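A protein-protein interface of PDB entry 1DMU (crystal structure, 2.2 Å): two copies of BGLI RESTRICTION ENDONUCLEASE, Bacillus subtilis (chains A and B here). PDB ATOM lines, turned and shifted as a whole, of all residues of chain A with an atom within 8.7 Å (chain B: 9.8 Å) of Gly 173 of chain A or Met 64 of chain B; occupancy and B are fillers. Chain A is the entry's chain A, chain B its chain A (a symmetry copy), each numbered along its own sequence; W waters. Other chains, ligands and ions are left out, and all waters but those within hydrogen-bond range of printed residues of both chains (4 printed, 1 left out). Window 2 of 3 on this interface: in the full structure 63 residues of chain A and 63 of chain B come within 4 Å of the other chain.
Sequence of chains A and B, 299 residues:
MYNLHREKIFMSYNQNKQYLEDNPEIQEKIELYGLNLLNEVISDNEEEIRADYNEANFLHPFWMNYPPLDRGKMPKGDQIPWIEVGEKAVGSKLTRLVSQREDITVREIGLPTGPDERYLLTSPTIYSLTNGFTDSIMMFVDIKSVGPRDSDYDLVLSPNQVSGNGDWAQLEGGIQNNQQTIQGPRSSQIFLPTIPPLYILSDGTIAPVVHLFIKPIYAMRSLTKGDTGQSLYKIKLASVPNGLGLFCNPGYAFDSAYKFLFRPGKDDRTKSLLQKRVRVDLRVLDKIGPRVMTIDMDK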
ATOM      1  N   TYR A   2      23.494 -11.031  -4.751  1.00  0.00           N
ATOM      2  CA  TYR A   2      24.461 -11.220  -5.830  1.00  0.00           C
ATOM      3  C   TYR A   2      25.496 -10.105  -5.985  1.00  0.00           C
ATOM      4  O   TYR A   2      26.652 -10.360  -6.365  1.00  0.00           O
ATOM      5  CB  TYR A   2      23.731 -11.382  -7.174  1.00  0.00           C
ATOM      6  CG  TYR A   2      22.929 -12.661  -7.341  1.00  0.00           C
ATOM      7  CD1 TYR A   2      23.044 -13.715  -6.437  1.00  0.00           C
ATOM      8  CD2 TYR A   2      22.047 -12.814  -8.414  1.00  0.00           C
ATOM      9  CE1 TYR A   2      22.298 -14.888  -6.602  1.00  0.00           C
ATOM     10  CE2 TYR A   2      21.307 -13.973  -8.581  1.00  0.00           C
ATOM     11  CZ  TYR A   2      21.434 -15.006  -7.672  1.00  0.00           C
ATOM     12  OH  TYR A   2      20.685 -16.155  -7.824  1.00  0.00           O
ATOM     13  N   ASN A   3      25.089  -8.879  -5.671  1.00  0.00           N
ATOM     14  CA  ASN A   3      25.966  -7.733  -5.837  1.00  0.00           C
ATOM     15  C   ASN A   3      26.623  -7.160  -4.581  1.00  0.00           C
ATOM     16  O   ASN A   3      27.578  -6.393  -4.689  1.00  0.00           O
ATOM     17  CB  ASN A   3      25.194  -6.620  -6.569  1.00  0.00           C
ATOM     18  CG  ASN A   3      24.791  -7.024  -7.989  1.00  0.00           C
ATOM     19  OD1 ASN A   3      25.492  -7.795  -8.661  1.00  0.00           O
ATOM     20  ND2 ASN A   3      23.656  -6.513  -8.447  1.00  0.00           N
ATOM     21  N   ARG A   6      30.164  -8.317  -4.478  1.00  0.00           N
ATOM     22  CA  ARG A   6      30.682  -8.565  -5.808  1.00  0.00           C
ATOM     23  C   ARG A   6      31.952  -7.822  -6.194  1.00  0.00           C
ATOM     24  O   ARG A   6      32.889  -8.442  -6.703  1.00  0.00           O
ATOM     25  CB  ARG A   6      29.592  -8.320  -6.864  1.00  0.00           C
ATOM     26  CG  ARG A   6      29.713  -9.270  -8.059  1.00  0.00           C
ATOM     27  CD  ARG A   6      28.921  -8.792  -9.267  1.00  0.00           C
ATOM     28  NE  ARG A   6      28.832  -9.828 -10.294  1.00  0.00           N
ATOM     29  CZ  ARG A   6      28.021 -10.883 -10.246  1.00  0.00           C
ATOM     30  NH1 ARG A   6      27.208 -11.077  -9.209  1.00  0.00           N
ATOM     31  NH2 ARG A   6      28.042 -11.769 -11.226  1.00  0.00           N
ATOM     32  N   PHE A  10      35.408  -9.611  -7.018  1.00  0.00           N
ATOM     33  CA  PHE A  10      35.893  -9.357  -8.371  1.00  0.00           C
ATOM     34  C   PHE A  10      37.342  -8.859  -8.379  1.00  0.00           C
ATOM     35  O   PHE A  10      38.207  -9.438  -9.036  1.00  0.00           O
ATOM     36  CB  PHE A  10      34.976  -8.323  -9.034  1.00  0.00           C
ATOM     37  CG  PHE A  10      35.372  -7.958 -10.430  1.00  0.00           C
ATOM     38  CD1 PHE A  10      35.585  -8.940 -11.383  1.00  0.00           C
ATOM     39  CD2 PHE A  10      35.519  -6.625 -10.795  1.00  0.00           C
ATOM     40  CE1 PHE A  10      35.941  -8.608 -12.681  1.00  0.00           C
ATOM     41  CE2 PHE A  10      35.877  -6.277 -12.098  1.00  0.00           C
ATOM     42  CZ  PHE A  10      36.089  -7.276 -13.043  1.00  0.00           C
ATOM     43  N   PRO A 112      25.927 -24.624  -5.480  1.00  0.00           N
ATOM     44  CA  PRO A 112      24.871 -25.381  -6.145  1.00  0.00           C
ATOM     45  C   PRO A 112      25.337 -26.564  -6.994  1.00  0.00           C
ATOM     46  O   PRO A 112      24.527 -27.422  -7.339  1.00  0.00           O
ATOM     47  CB  PRO A 112      24.170 -24.324  -6.992  1.00  0.00           C
ATOM     48  CG  PRO A 112      25.270 -23.381  -7.376  1.00  0.00           C
ATOM     49  CD  PRO A 112      26.227 -23.367  -6.200  1.00  0.00           C
ATOM     50  N   THR A 113      26.622 -26.610  -7.344  1.00  0.00           N
ATOM     51  CA  THR A 113      27.150 -27.704  -8.160  1.00  0.00           C
ATOM     52  C   THR A 113      28.524 -28.108  -7.697  1.00  0.00           C
ATOM     53  O   THR A 113      29.165 -27.392  -6.939  1.00  0.00           O
ATOM     54  CB  THR A 113      27.314 -27.308  -9.655  1.00  0.00           C
ATOM     55  OG1 THR A 113      28.343 -26.305  -9.776  1.00  0.00           O
ATOM     56  CG2 THR A 113      25.997 -26.791 -10.234  1.00  0.00           C
ATOM     57  N   ASP A 167      38.291 -16.858 -16.720  1.00  0.00           N
ATOM     58  CA  ASP A 167      38.391 -15.425 -16.960  1.00  0.00           C
ATOM     59  C   ASP A 167      37.107 -14.768 -16.480  1.00  0.00           C
ATOM     60  O   ASP A 167      36.032 -15.325 -16.629  1.00  0.00           O
ATOM     61  CB  ASP A 167      38.594 -15.133 -18.450  1.00  0.00           C
ATOM     62  CG  ASP A 167      39.927 -15.654 -18.968  1.00  0.00           C
ATOM     63  OD1 ASP A 167      40.849 -15.866 -18.149  1.00  0.00           O
ATOM     64  OD2 ASP A 167      40.049 -15.855 -20.194  1.00  0.00           O
ATOM     65  N   TRP A 168      37.237 -13.588 -15.885  1.00  0.00           N
ATOM     66  CA  TRP A 168      36.097 -12.825 -15.396  1.00  0.00           C
ATOM     67  C   TRP A 168      36.372 -11.403 -15.897  1.00  0.00           C
ATOM     68  O   TRP A 168      36.997 -10.595 -15.215  1.00  0.00           O
ATOM     69  CB  TRP A 168      36.033 -12.903 -13.856  1.00  0.00           C
ATOM     70  CG  TRP A 168      34.843 -12.191 -13.206  1.00  0.00           C
ATOM     71  CD1 TRP A 168      33.907 -11.426 -13.833  1.00  0.00           C
ATOM     72  CD2 TRP A 168      34.522 -12.145 -11.794  1.00  0.00           C
ATOM     73  NE1 TRP A 168      33.026 -10.899 -12.910  1.00  0.00           N
ATOM     74  CE2 TRP A 168      33.378 -11.322 -11.656  1.00  0.00           C
ATOM     75  CE3 TRP A 168      35.093 -12.716 -10.638  1.00  0.00           C
ATOM     76  CZ2 TRP A 168      32.787 -11.049 -10.403  1.00  0.00           C
ATOM     77  CZ3 TRP A 168      34.508 -12.442  -9.390  1.00  0.00           C
ATOM     78  CH2 TRP A 168      33.365 -11.614  -9.287  1.00  0.00           C
ATOM     79  N   ALA A 169      35.913 -11.123 -17.112  1.00  0.00           N
ATOM     80  CA  ALA A 169      36.133  -9.832 -17.759  1.00  0.00           C
ATOM     81  C   ALA A 169      35.532  -8.627 -17.047  1.00  0.00           C
ATOM     82  O   ALA A 169      36.266  -7.713 -16.634  1.00  0.00           O
ATOM     83  CB  ALA A 169      35.615  -9.884 -19.207  1.00  0.00           C
ATOM     84  N   GLN A 170      34.202  -8.626 -16.916  1.00  0.00           N
ATOM     85  CA  GLN A 170      33.481  -7.523 -16.287  1.00  0.00           C
ATOM     86  C   GLN A 170      32.797  -7.900 -14.981  1.00  0.00           C
ATOM     87  O   GLN A 170      32.354  -9.030 -14.806  1.00  0.00           O
ATOM     88  CB  GLN A 170      32.449  -6.969 -17.266  1.00  0.00           C
ATOM     89  CG  GLN A 170      33.056  -6.408 -18.566  1.00  0.00           C
ATOM     90  CD  GLN A 170      33.696  -5.031 -18.373  1.00  0.00           C
ATOM     91  OE1 GLN A 170      33.483  -4.363 -17.342  1.00  0.00           O
ATOM     92  NE2 GLN A 170      34.478  -4.594 -19.358  1.00  0.00           N
ATOM     93  N   LEU A 171      32.692  -6.922 -14.088  1.00  0.00           N
ATOM     94  CA  LEU A 171      32.075  -7.085 -12.774  1.00  0.00           C
ATOM     95  C   LEU A 171      30.653  -7.652 -12.776  1.00  0.00           C
ATOM     96  O   LEU A 171      30.380  -8.625 -12.080  1.00  0.00           O
ATOM     97  CB  LEU A 171      32.080  -5.742 -12.043  1.00  0.00           C
ATOM     98  CG  LEU A 171      31.323  -5.696 -10.718  1.00  0.00           C
ATOM     99  CD1 LEU A 171      32.173  -6.227  -9.570  1.00  0.00           C
ATOM    100  CD2 LEU A 171      30.913  -4.285 -10.485  1.00  0.00           C
ATOM    101  N   GLU A 172      29.747  -7.037 -13.530  1.00  0.00           N
ATOM    102  CA  GLU A 172      28.377  -7.528 -13.577  1.00  0.00           C
ATOM    103  C   GLU A 172      28.339  -8.904 -14.237  1.00  0.00           C
ATOM    104  O   GLU A 172      27.285  -9.536 -14.315  1.00  0.00           O
ATOM    105  CB  GLU A 172      27.481  -6.539 -14.333  1.00  0.00           C
ATOM    106  N   GLY A 173      29.496  -9.353 -14.714  1.00  0.00           N
ATOM    107  CA  GLY A 173      29.589 -10.663 -15.344  1.00  0.00           C
ATOM    108  C   GLY A 173      30.129 -11.696 -14.357  1.00  0.00           C
ATOM    109  O   GLY A 173      30.061 -11.493 -13.146  1.00  0.00           O
ATOM    110  N   GLY A 174      30.678 -12.794 -14.864  1.00  0.00           N
ATOM    111  CA  GLY A 174      31.213 -13.825 -13.987  1.00  0.00           C
ATOM    112  C   GLY A 174      32.345 -14.631 -14.597  1.00  0.00           C
ATOM    113  O   GLY A 174      32.835 -14.299 -15.673  1.00  0.00           O
ATOM    114  N   ILE A 175      32.775 -15.691 -13.922  1.00  0.00           N
ATOM    115  CA  ILE A 175      33.852 -16.486 -14.467  1.00  0.00           C
ATOM    116  C   ILE A 175      33.351 -17.301 -15.646  1.00  0.00           C
ATOM    117  O   ILE A 175      32.197 -17.740 -15.678  1.00  0.00           O
ATOM    118  CB  ILE A 175      34.503 -17.439 -13.402  1.00  0.00           C
ATOM    119  CG1 ILE A 175      33.648 -18.702 -13.204  1.00  0.00           C
ATOM    120  CG2 ILE A 175      34.731 -16.665 -12.088  1.00  0.00           C
ATOM    121  CD1 ILE A 175      34.139 -19.960 -13.944  1.00  0.00           C
ATOM    122  N   GLN A 176      34.229 -17.472 -16.626  1.00  0.00           N
ATOM    123  CA  GLN A 176      33.913 -18.250 -17.809  1.00  0.00           C
ATOM    124  C   GLN A 176      35.138 -19.066 -18.152  1.00  0.00           C
ATOM    125  O   GLN A 176      36.278 -18.574 -18.049  1.00  0.00           O
ATOM    126  CB  GLN A 176      33.583 -17.347 -18.991  1.00  0.00           C
ATOM    127  CG  GLN A 176      32.291 -16.600 -18.877  1.00  0.00           C
ATOM    128  CD  GLN A 176      32.124 -15.604 -20.006  1.00  0.00           C
ATOM    129  OE1 GLN A 176      32.024 -14.388 -19.779  1.00  0.00           O
ATOM    130  NE2 GLN A 176      32.095 -16.109 -21.237  1.00  0.00           N
ATOM    131  N   THR A 194      33.252 -26.284 -15.657  1.00  0.00           N
ATOM    132  CA  THR A 194      32.374 -25.243 -15.141  1.00  0.00           C
ATOM    133  C   THR A 194      32.885 -24.634 -13.842  1.00  0.00           C
ATOM    134  O   THR A 194      32.330 -23.650 -13.355  1.00  0.00           O
ATOM    135  CB  THR A 194      30.973 -25.809 -14.828  1.00  0.00           C
ATOM    136  OG1 THR A 194      31.110 -26.897 -13.904  1.00  0.00           O
ATOM    137  CG2 THR A 194      30.271 -26.291 -16.099  1.00  0.00           C
ATOM    138  N   PRO A 196      35.592 -22.666 -11.368  1.00  0.00           N
ATOM    139  CA  PRO A 196      36.652 -21.651 -11.442  1.00  0.00           C
ATOM    140  C   PRO A 196      37.916 -22.222 -10.804  1.00  0.00           C
ATOM    141  O   PRO A 196      37.829 -23.095  -9.945  1.00  0.00           O
ATOM    142  CB  PRO A 196      36.095 -20.502 -10.624  1.00  0.00           C
ATOM    143  CG  PRO A 196      35.238 -21.155  -9.616  1.00  0.00           C
ATOM    144  CD  PRO A 196      34.587 -22.313 -10.345  1.00  0.00           C
ATOM    145  N   ALA B  56      26.403 -19.274  -0.879  1.00  0.00           N
ATOM    146  CA  ALA B  56      26.231 -19.720  -2.268  1.00  0.00           C
ATOM    147  C   ALA B  56      25.793 -18.575  -3.182  1.00  0.00           C
ATOM    148  O   ALA B  56      26.153 -18.534  -4.355  1.00  0.00           O
ATOM    149  CB  ALA B  56      25.197 -20.855  -2.327  1.00  0.00           C
ATOM    150  N   ASN B  57      24.995 -17.661  -2.639  1.00  0.00           N
ATOM    151  CA  ASN B  57      24.490 -16.497  -3.383  1.00  0.00           C
ATOM    152  C   ASN B  57      25.571 -15.449  -3.636  1.00  0.00           C
ATOM    153  O   ASN B  57      25.571 -14.788  -4.679  1.00  0.00           O
ATOM    154  CB  ASN B  57      23.368 -15.819  -2.608  1.00  0.00           C
ATOM    155  CG  ASN B  57      22.195 -16.736  -2.359  1.00  0.00           C
ATOM    156  OD1 ASN B  57      21.453 -17.085  -3.286  1.00  0.00           O
ATOM    157  ND2 ASN B  57      22.011 -17.124  -1.101  1.00  0.00           N
ATOM    158  N   PHE B  58      26.468 -15.284  -2.663  1.00  0.00           N
ATOM    159  CA  PHE B  58      27.554 -14.321  -2.776  1.00  0.00           C
ATOM    160  C   PHE B  58      28.573 -14.838  -3.802  1.00  0.00           C
ATOM    161  O   PHE B  58      29.250 -14.054  -4.486  1.00  0.00           O
ATOM    162  CB  PHE B  58      28.196 -14.113  -1.395  1.00  0.00           C
ATOM    163  CG  PHE B  58      27.239 -13.557  -0.354  1.00  0.00           C
ATOM    164  CD1 PHE B  58      27.352 -13.924   0.988  1.00  0.00           C
ATOM    165  CD2 PHE B  58      26.238 -12.662  -0.707  1.00  0.00           C
ATOM    166  CE1 PHE B  58      26.497 -13.411   1.944  1.00  0.00           C
ATOM    167  CE2 PHE B  58      25.369 -12.142   0.257  1.00  0.00           C
ATOM    168  CZ  PHE B  58      25.503 -12.518   1.580  1.00  0.00           C
ATOM    169  N   LEU B  59      28.647 -16.164  -3.918  1.00  0.00           N
ATOM    170  CA  LEU B  59      29.552 -16.832  -4.850  1.00  0.00           C
ATOM    171  C   LEU B  59      28.936 -16.908  -6.259  1.00  0.00           C
ATOM    172  O   LEU B  59      29.502 -17.547  -7.157  1.00  0.00           O
ATOM    173  CB  LEU B  59      29.888 -18.239  -4.332  1.00  0.00           C
ATOM    174  CG  LEU B  59      30.699 -18.258  -3.023  1.00  0.00           C
ATOM    175  CD1 LEU B  59      31.059 -19.690  -2.629  1.00  0.00           C
ATOM    176  CD2 LEU B  59      31.980 -17.412  -3.213  1.00  0.00           C
ATOM    177  N   HIS B  60      27.802 -16.222  -6.437  1.00  0.00           N
ATOM    178  CA  HIS B  60      27.055 -16.158  -7.702  1.00  0.00           C
ATOM    179  C   HIS B  60      27.934 -16.016  -8.957  1.00  0.00           C
ATOM    180  O   HIS B  60      27.742 -16.743  -9.935  1.00  0.00           O
ATOM    181  CB  HIS B  60      26.041 -15.004  -7.649  1.00  0.00           C
ATOM    182  CG  HIS B  60      25.364 -14.706  -8.961  1.00  0.00           C
ATOM    183  ND1 HIS B  60      25.599 -13.546  -9.675  1.00  0.00           N
ATOM    184  CD2 HIS B  60      24.424 -15.387  -9.661  1.00  0.00           C
ATOM    185  CE1 HIS B  60      24.837 -13.528 -10.753  1.00  0.00           C
ATOM    186  NE2 HIS B  60      24.114 -14.632 -10.769  1.00  0.00           N
ATOM    187  N   PRO B  61      28.893 -15.066  -8.956  1.00  0.00           N
ATOM    188  CA  PRO B  61      29.751 -14.907 -10.134  1.00  0.00           C
ATOM    189  C   PRO B  61      30.486 -16.177 -10.510  1.00  0.00           C
ATOM    190  O   PRO B  61      30.808 -16.402 -11.685  1.00  0.00           O
ATOM    191  CB  PRO B  61      30.749 -13.812  -9.727  1.00  0.00           C
ATOM    192  CG  PRO B  61      30.654 -13.715  -8.243  1.00  0.00           C
ATOM    193  CD  PRO B  61      29.227 -14.082  -7.910  1.00  0.00           C
ATOM    194  N   PHE B  62      30.759 -17.015  -9.515  1.00  0.00           N
ATOM    195  CA  PHE B  62      31.508 -18.233  -9.780  1.00  0.00           C
ATOM    196  C   PHE B  62      30.717 -19.346 -10.478  1.00  0.00           C
ATOM    197  O   PHE B  62      31.313 -20.250 -11.078  1.00  0.00           O
ATOM    198  CB  PHE B  62      32.149 -18.724  -8.477  1.00  0.00           C
ATOM    199  CG  PHE B  62      33.149 -17.753  -7.901  1.00  0.00           C
ATOM    200  CD1 PHE B  62      32.861 -17.043  -6.737  1.00  0.00           C
ATOM    201  CD2 PHE B  62      34.370 -17.523  -8.553  1.00  0.00           C
ATOM    202  CE1 PHE B  62      33.772 -16.107  -6.225  1.00  0.00           C
ATOM    203  CE2 PHE B  62      35.291 -16.595  -8.057  1.00  0.00           C
ATOM    204  CZ  PHE B  62      34.995 -15.883  -6.890  1.00  0.00           C
ATOM    205  N   TRP B  63      29.383 -19.266 -10.424  1.00  0.00           N
ATOM    206  CA  TRP B  63      28.532 -20.274 -11.052  1.00  0.00           C
ATOM    207  C   TRP B  63      27.438 -19.711 -11.984  1.00  0.00           C
ATOM    208  O   TRP B  63      26.771 -20.467 -12.691  1.00  0.00           O
ATOM    209  CB  TRP B  63      27.885 -21.158  -9.976  1.00  0.00           C
ATOM    210  CG  TRP B  63      27.150 -20.407  -8.862  1.00  0.00           C
ATOM    211  CD1 TRP B  63      27.623 -20.147  -7.602  1.00  0.00           C
ATOM    212  CD2 TRP B  63      25.801 -19.897  -8.891  1.00  0.00           C
ATOM    213  NE1 TRP B  63      26.659 -19.516  -6.851  1.00  0.00           N
ATOM    214  CE2 TRP B  63      25.532 -19.349  -7.614  1.00  0.00           C
ATOM    215  CE3 TRP B  63      24.795 -19.854  -9.869  1.00  0.00           C
ATOM    216  CZ2 TRP B  63      24.304 -18.764  -7.288  1.00  0.00           C
ATOM    217  CZ3 TRP B  63      23.571 -19.268  -9.539  1.00  0.00           C
ATOM    218  CH2 TRP B  63      23.338 -18.731  -8.255  1.00  0.00           C
ATOM    219  N   MET B  64      27.265 -18.397 -12.003  1.00  0.00           N
ATOM    220  CA  MET B  64      26.241 -17.783 -12.849  1.00  0.00           C
ATOM    221  C   MET B  64      26.214 -18.239 -14.313  1.00  0.00           C
ATOM    222  O   MET B  64      25.143 -18.375 -14.889  1.00  0.00           O
ATOM    223  CB  MET B  64      26.349 -16.252 -12.800  1.00  0.00           C
ATOM    224  CG  MET B  64      27.336 -15.650 -13.780  1.00  0.00           C
ATOM    225  SD  MET B  64      27.345 -13.860 -13.603  1.00  0.00           S
ATOM    226  CE  MET B  64      25.886 -13.431 -14.396  1.00  0.00           C
ATOM    227  N   ASN B  65      27.377 -18.475 -14.918  1.00  0.00           N
ATOM    228  CA  ASN B  65      27.426 -18.904 -16.316  1.00  0.00           C
ATOM    229  C   ASN B  65      27.251 -20.412 -16.502  1.00  0.00           C
ATOM    230  O   ASN B  65      27.084 -20.884 -17.628  1.00  0.00           O
ATOM    231  CB  ASN B  65      28.747 -18.454 -16.949  1.00  0.00           C
ATOM    232  CG  ASN B  65      28.827 -16.943 -17.112  1.00  0.00           C
ATOM    233  OD1 ASN B  65      27.807 -16.273 -17.258  1.00  0.00           O
ATOM    234  ND2 ASN B  65      30.035 -16.401 -17.082  1.00  0.00           N
ATOM    235  N   TYR B  66      27.292 -21.162 -15.395  1.00  0.00           N
ATOM    236  CA  TYR B  66      27.139 -22.625 -15.404  1.00  0.00           C
ATOM    237  C   TYR B  66      26.224 -23.071 -14.262  1.00  0.00           C
ATOM    238  O   TYR B  66      26.597 -23.905 -13.431  1.00  0.00           O
ATOM    239  CB  TYR B  66      28.495 -23.306 -15.235  1.00  0.00           C
ATOM    240  CG  TYR B  66      29.545 -22.775 -16.159  1.00  0.00           C
ATOM    241  CD1 TYR B  66      30.510 -21.899 -15.697  1.00  0.00           C
ATOM    242  CD2 TYR B  66      29.553 -23.116 -17.515  1.00  0.00           C
ATOM    243  CE1 TYR B  66      31.464 -21.355 -16.562  1.00  0.00           C
ATOM    244  CE2 TYR B  66      30.509 -22.579 -18.393  1.00  0.00           C
ATOM    245  CZ  TYR B  66      31.461 -21.694 -17.902  1.00  0.00           C
ATOM    246  OH  TYR B  66      32.413 -21.122 -18.728  1.00  0.00           O
ATOM    247  N   PRO B  67      24.999 -22.542 -14.225  1.00  0.00           N
ATOM    248  CA  PRO B  67      24.078 -22.916 -13.162  1.00  0.00           C
ATOM    249  C   PRO B  67      23.493 -24.282 -13.446  1.00  0.00           C
ATOM    250  O   PRO B  67      23.629 -24.800 -14.557  1.00  0.00           O
ATOM    251  CB  PRO B  67      23.002 -21.852 -13.260  1.00  0.00           C
ATOM    252  CG  PRO B  67      22.925 -21.616 -14.766  1.00  0.00           C
ATOM    253  CD  PRO B  67      24.371 -21.618 -15.188  1.00  0.00           C
ATOM    254  N   PRO B  68      22.881 -24.916 -12.433  1.00  0.00           N
ATOM    255  CA  PRO B  68      22.285 -26.221 -12.735  1.00  0.00           C
ATOM    256  C   PRO B  68      21.144 -25.832 -13.689  1.00  0.00           C
ATOM    257  O   PRO B  68      20.455 -24.837 -13.444  1.00  0.00           O
ATOM    258  CB  PRO B  68      21.737 -26.702 -11.386  1.00  0.00           C
ATOM    259  CG  PRO B  68      22.418 -25.836 -10.350  1.00  0.00           C
ATOM    260  CD  PRO B  68      22.707 -24.531 -11.023  1.00  0.00           C
ATOM    261  N   LEU B  69      20.935 -26.577 -14.766  1.00  0.00           N
ATOM    262  CA  LEU B  69      19.879 -26.199 -15.703  1.00  0.00           C
ATOM    263  C   LEU B  69      18.510 -26.433 -15.067  1.00  0.00           C
ATOM    264  O   LEU B  69      18.397 -27.178 -14.086  1.00  0.00           O
ATOM    265  CB  LEU B  69      20.015 -26.991 -17.010  1.00  0.00           C
ATOM    266  CG  LEU B  69      21.265 -26.719 -17.887  1.00  0.00           C
ATOM    267  CD1 LEU B  69      21.218 -27.631 -19.115  1.00  0.00           C
ATOM    268  CD2 LEU B  69      21.355 -25.235 -18.317  1.00  0.00           C
ATOM    269  N   ILE B  80      17.023 -20.828  -9.202  1.00  0.00           N
ATOM    270  CA  ILE B  80      18.211 -21.625  -9.459  1.00  0.00           C
ATOM    271  C   ILE B  80      18.089 -22.937  -8.666  1.00  0.00           C
ATOM    272  O   ILE B  80      17.901 -22.898  -7.458  1.00  0.00           O
ATOM    273  CB  ILE B  80      19.479 -20.902  -8.996  1.00  0.00           C
ATOM    274  CG1 ILE B  80      19.560 -19.522  -9.644  1.00  0.00           C
ATOM    275  CG2 ILE B  80      20.703 -21.759  -9.319  1.00  0.00           C
ATOM    276  CD1 ILE B  80      19.979 -19.557 -11.106  1.00  0.00           C
ATOM    277  N   TRP B  82      18.375 -25.300  -6.206  1.00  0.00           N
ATOM    278  CA  TRP B  82      19.097 -25.140  -4.938  1.00  0.00           C
ATOM    279  C   TRP B  82      19.350 -26.393  -4.105  1.00  0.00           C
ATOM    280  O   TRP B  82      19.776 -26.299  -2.955  1.00  0.00           O
ATOM    281  CB  TRP B  82      18.345 -24.102  -4.091  1.00  0.00           C
ATOM    282  CG  TRP B  82      19.196 -23.008  -3.492  1.00  0.00           C
ATOM    283  CD1 TRP B  82      19.094 -22.507  -2.235  1.00  0.00           C
ATOM    284  CD2 TRP B  82      20.244 -22.254  -4.138  1.00  0.00           C
ATOM    285  NE1 TRP B  82      19.997 -21.493  -2.045  1.00  0.00           N
ATOM    286  CE2 TRP B  82      20.717 -21.314  -3.196  1.00  0.00           C
ATOM    287  CE3 TRP B  82      20.822 -22.280  -5.420  1.00  0.00           C
ATOM    288  CZ2 TRP B  82      21.744 -20.407  -3.487  1.00  0.00           C
ATOM    289  CZ3 TRP B  82      21.846 -21.378  -5.710  1.00  0.00           C
ATOM    290  CH2 TRP B  82      22.294 -20.451  -4.741  1.00  0.00           C
HETATM  291  O   HOH W   1      30.188 -18.060 -13.860  1.00  0.00           O
HETATM  292  O   HOH W   2      28.949 -11.364  -5.488  1.00  0.00           O
HETATM  293  O   HOH W   3      30.268 -13.376 -17.416  1.00  0.00           O
HETATM  294  O   HOH W   4      28.504 -24.714 -11.616  1.00  0.00           O
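The backbone carbonyl oxygen of Gly 173 of chain A sits close to the side-chain sulfur of Met 64 of chain B (3.6 Å). The side-chain sulfur of Met 64 of chain B lies within hydrogen-bond range of the guanidinium group of Arg 6 of chain A (3.2 Å). The side-chain amide nitrogen (ND2) of Asn 65 of chain B is in hydrogen-bond range of the backbone carbonyl oxygen (O) of Ile 175 of chain A (2.9 Å). O of Pro 61 of chain B sits at hydrogen-bond distance from N of Ile 175 of chain A, 3.1 Å away. ND1 of His 60 of chain B lies within hydrogen-bond range of NH1 of Arg 6 of chain A, 3.0 Å away. The backbone NH (N) of Gly 174 of chain A lies within hydrogen-bond range of the side-chain sulfur (SD) of Met 64 of chain B, 3.7 Å away.
The backbone carbonyl oxygen (O) of Tyr 2 of chain A sits at hydrogen-bond distance from the guanidinium group (NH1) of Arg 6 of chain A, 3.0 Å away. The guanidinium group (NE) of Arg 6 of chain A sits at hydrogen-bond distance from the backbone carbonyl oxygen (O) of Leu 171 of chain A (2.7 Å).
Among the printed residues, merely in contact across the chains: Gln 176 of chain A with Asn 65 of chain B (2.9 Å), Tyr 2 of chain A with Asn 57 of chain B (3.3 Å), Gln 176 of chain A with Tyr 66 of chain B (3.4 Å), Thr 194 of chain A with Tyr 66 of chain B (3.4 Å), Trp 168 of chain A with Pro 61 of chain B (3.4 Å), Gly 174 of chain A with Pro 61 of chain B (3.5 Å), Tyr 2 of chain A with His 60 of chain B (3.5 Å), Ile 175 of chain A with Phe 62 of chain B (3.5 Å), Thr 113 of chain A with Pro 68 of chain B (3.7 Å), Arg 6 of chain A with Pro 61 of chain B (3.7 Å), Tyr 2 of chain A with Trp 63 of chain B (3.7 Å), Gly 174 of chain A with Asn 65 of chain B (3.8 Å), Pro 112 of chain A with Trp 63 of chain B (3.8 Å), Ile 175 of chain A with Tyr 66 of chain B (3.8 Å), Pro 196 of chain A with Phe 62 of chain B (3.9 Å), Pro 112 of chain A with Trp 82 of chain B (3.97 Å) and Tyr 2 of chain A with Ile 80 of chain B (3.99 Å).
Gly 173 of chain A touches one residue of chain B. Met 64 of chain B touches just these residues of chain A: Arg 6, Gly 173 and Gly 174. Gly 174 of chain A touches just these residues of chain B: Pro 61, Met 64 and Asn 65. Asn 65 of chain B touches just these residues of chain A: Gly 174, Ile 175 and Gln 176. Of the printed residues of chain A, Pro 68 of chain B touches Thr 113. Of the printed residues of chain A, Pro 61 of chain B touches Arg 6 (3.7 Å), Trp 168 (3.4 Å), Gly 174 (3.5 Å) and Ile 175 (3.1 Å). Leu 69 of chain B touches none of the printed residues of chain A. The nearest residue of chain A that does not touch Met 64 of chain B is Glu 172 of chain A (4.1 Å). The nearest printed residue of chain B that does not touch Gln 176 of chain A is Pro 61 of chain B (6.1 Å).
Of the 18 printed residues of chain A, 11 touch a printed residue of chain B. Along chain A the printed residues that touch a printed residue of chain B span positions 2 to 196. Of the 16 printed residues of chain B, 11 touch a printed residue of chain A. Among the printed residues, 23 pairs touch across the chains. Among the printed residues, no Asp or Glu carboxylate lies within 4 Å of a Lys or Arg side-chain nitrogen of the other chain.
No position is printed for both chains.
Water W4 bridges the side-chain hydroxyl (OG1) of Thr 113 of chain A and the backbone carbonyl oxygen (O) of Tyr 66 of chain B. Water W3 lies within hydrogen-bond range of N of Gly 174 of chain A (2.6 Å), ND2 of Asn 65 of chain B (3.1 Å) and OE1 of Gln 176 of chain A (3.1 Å).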
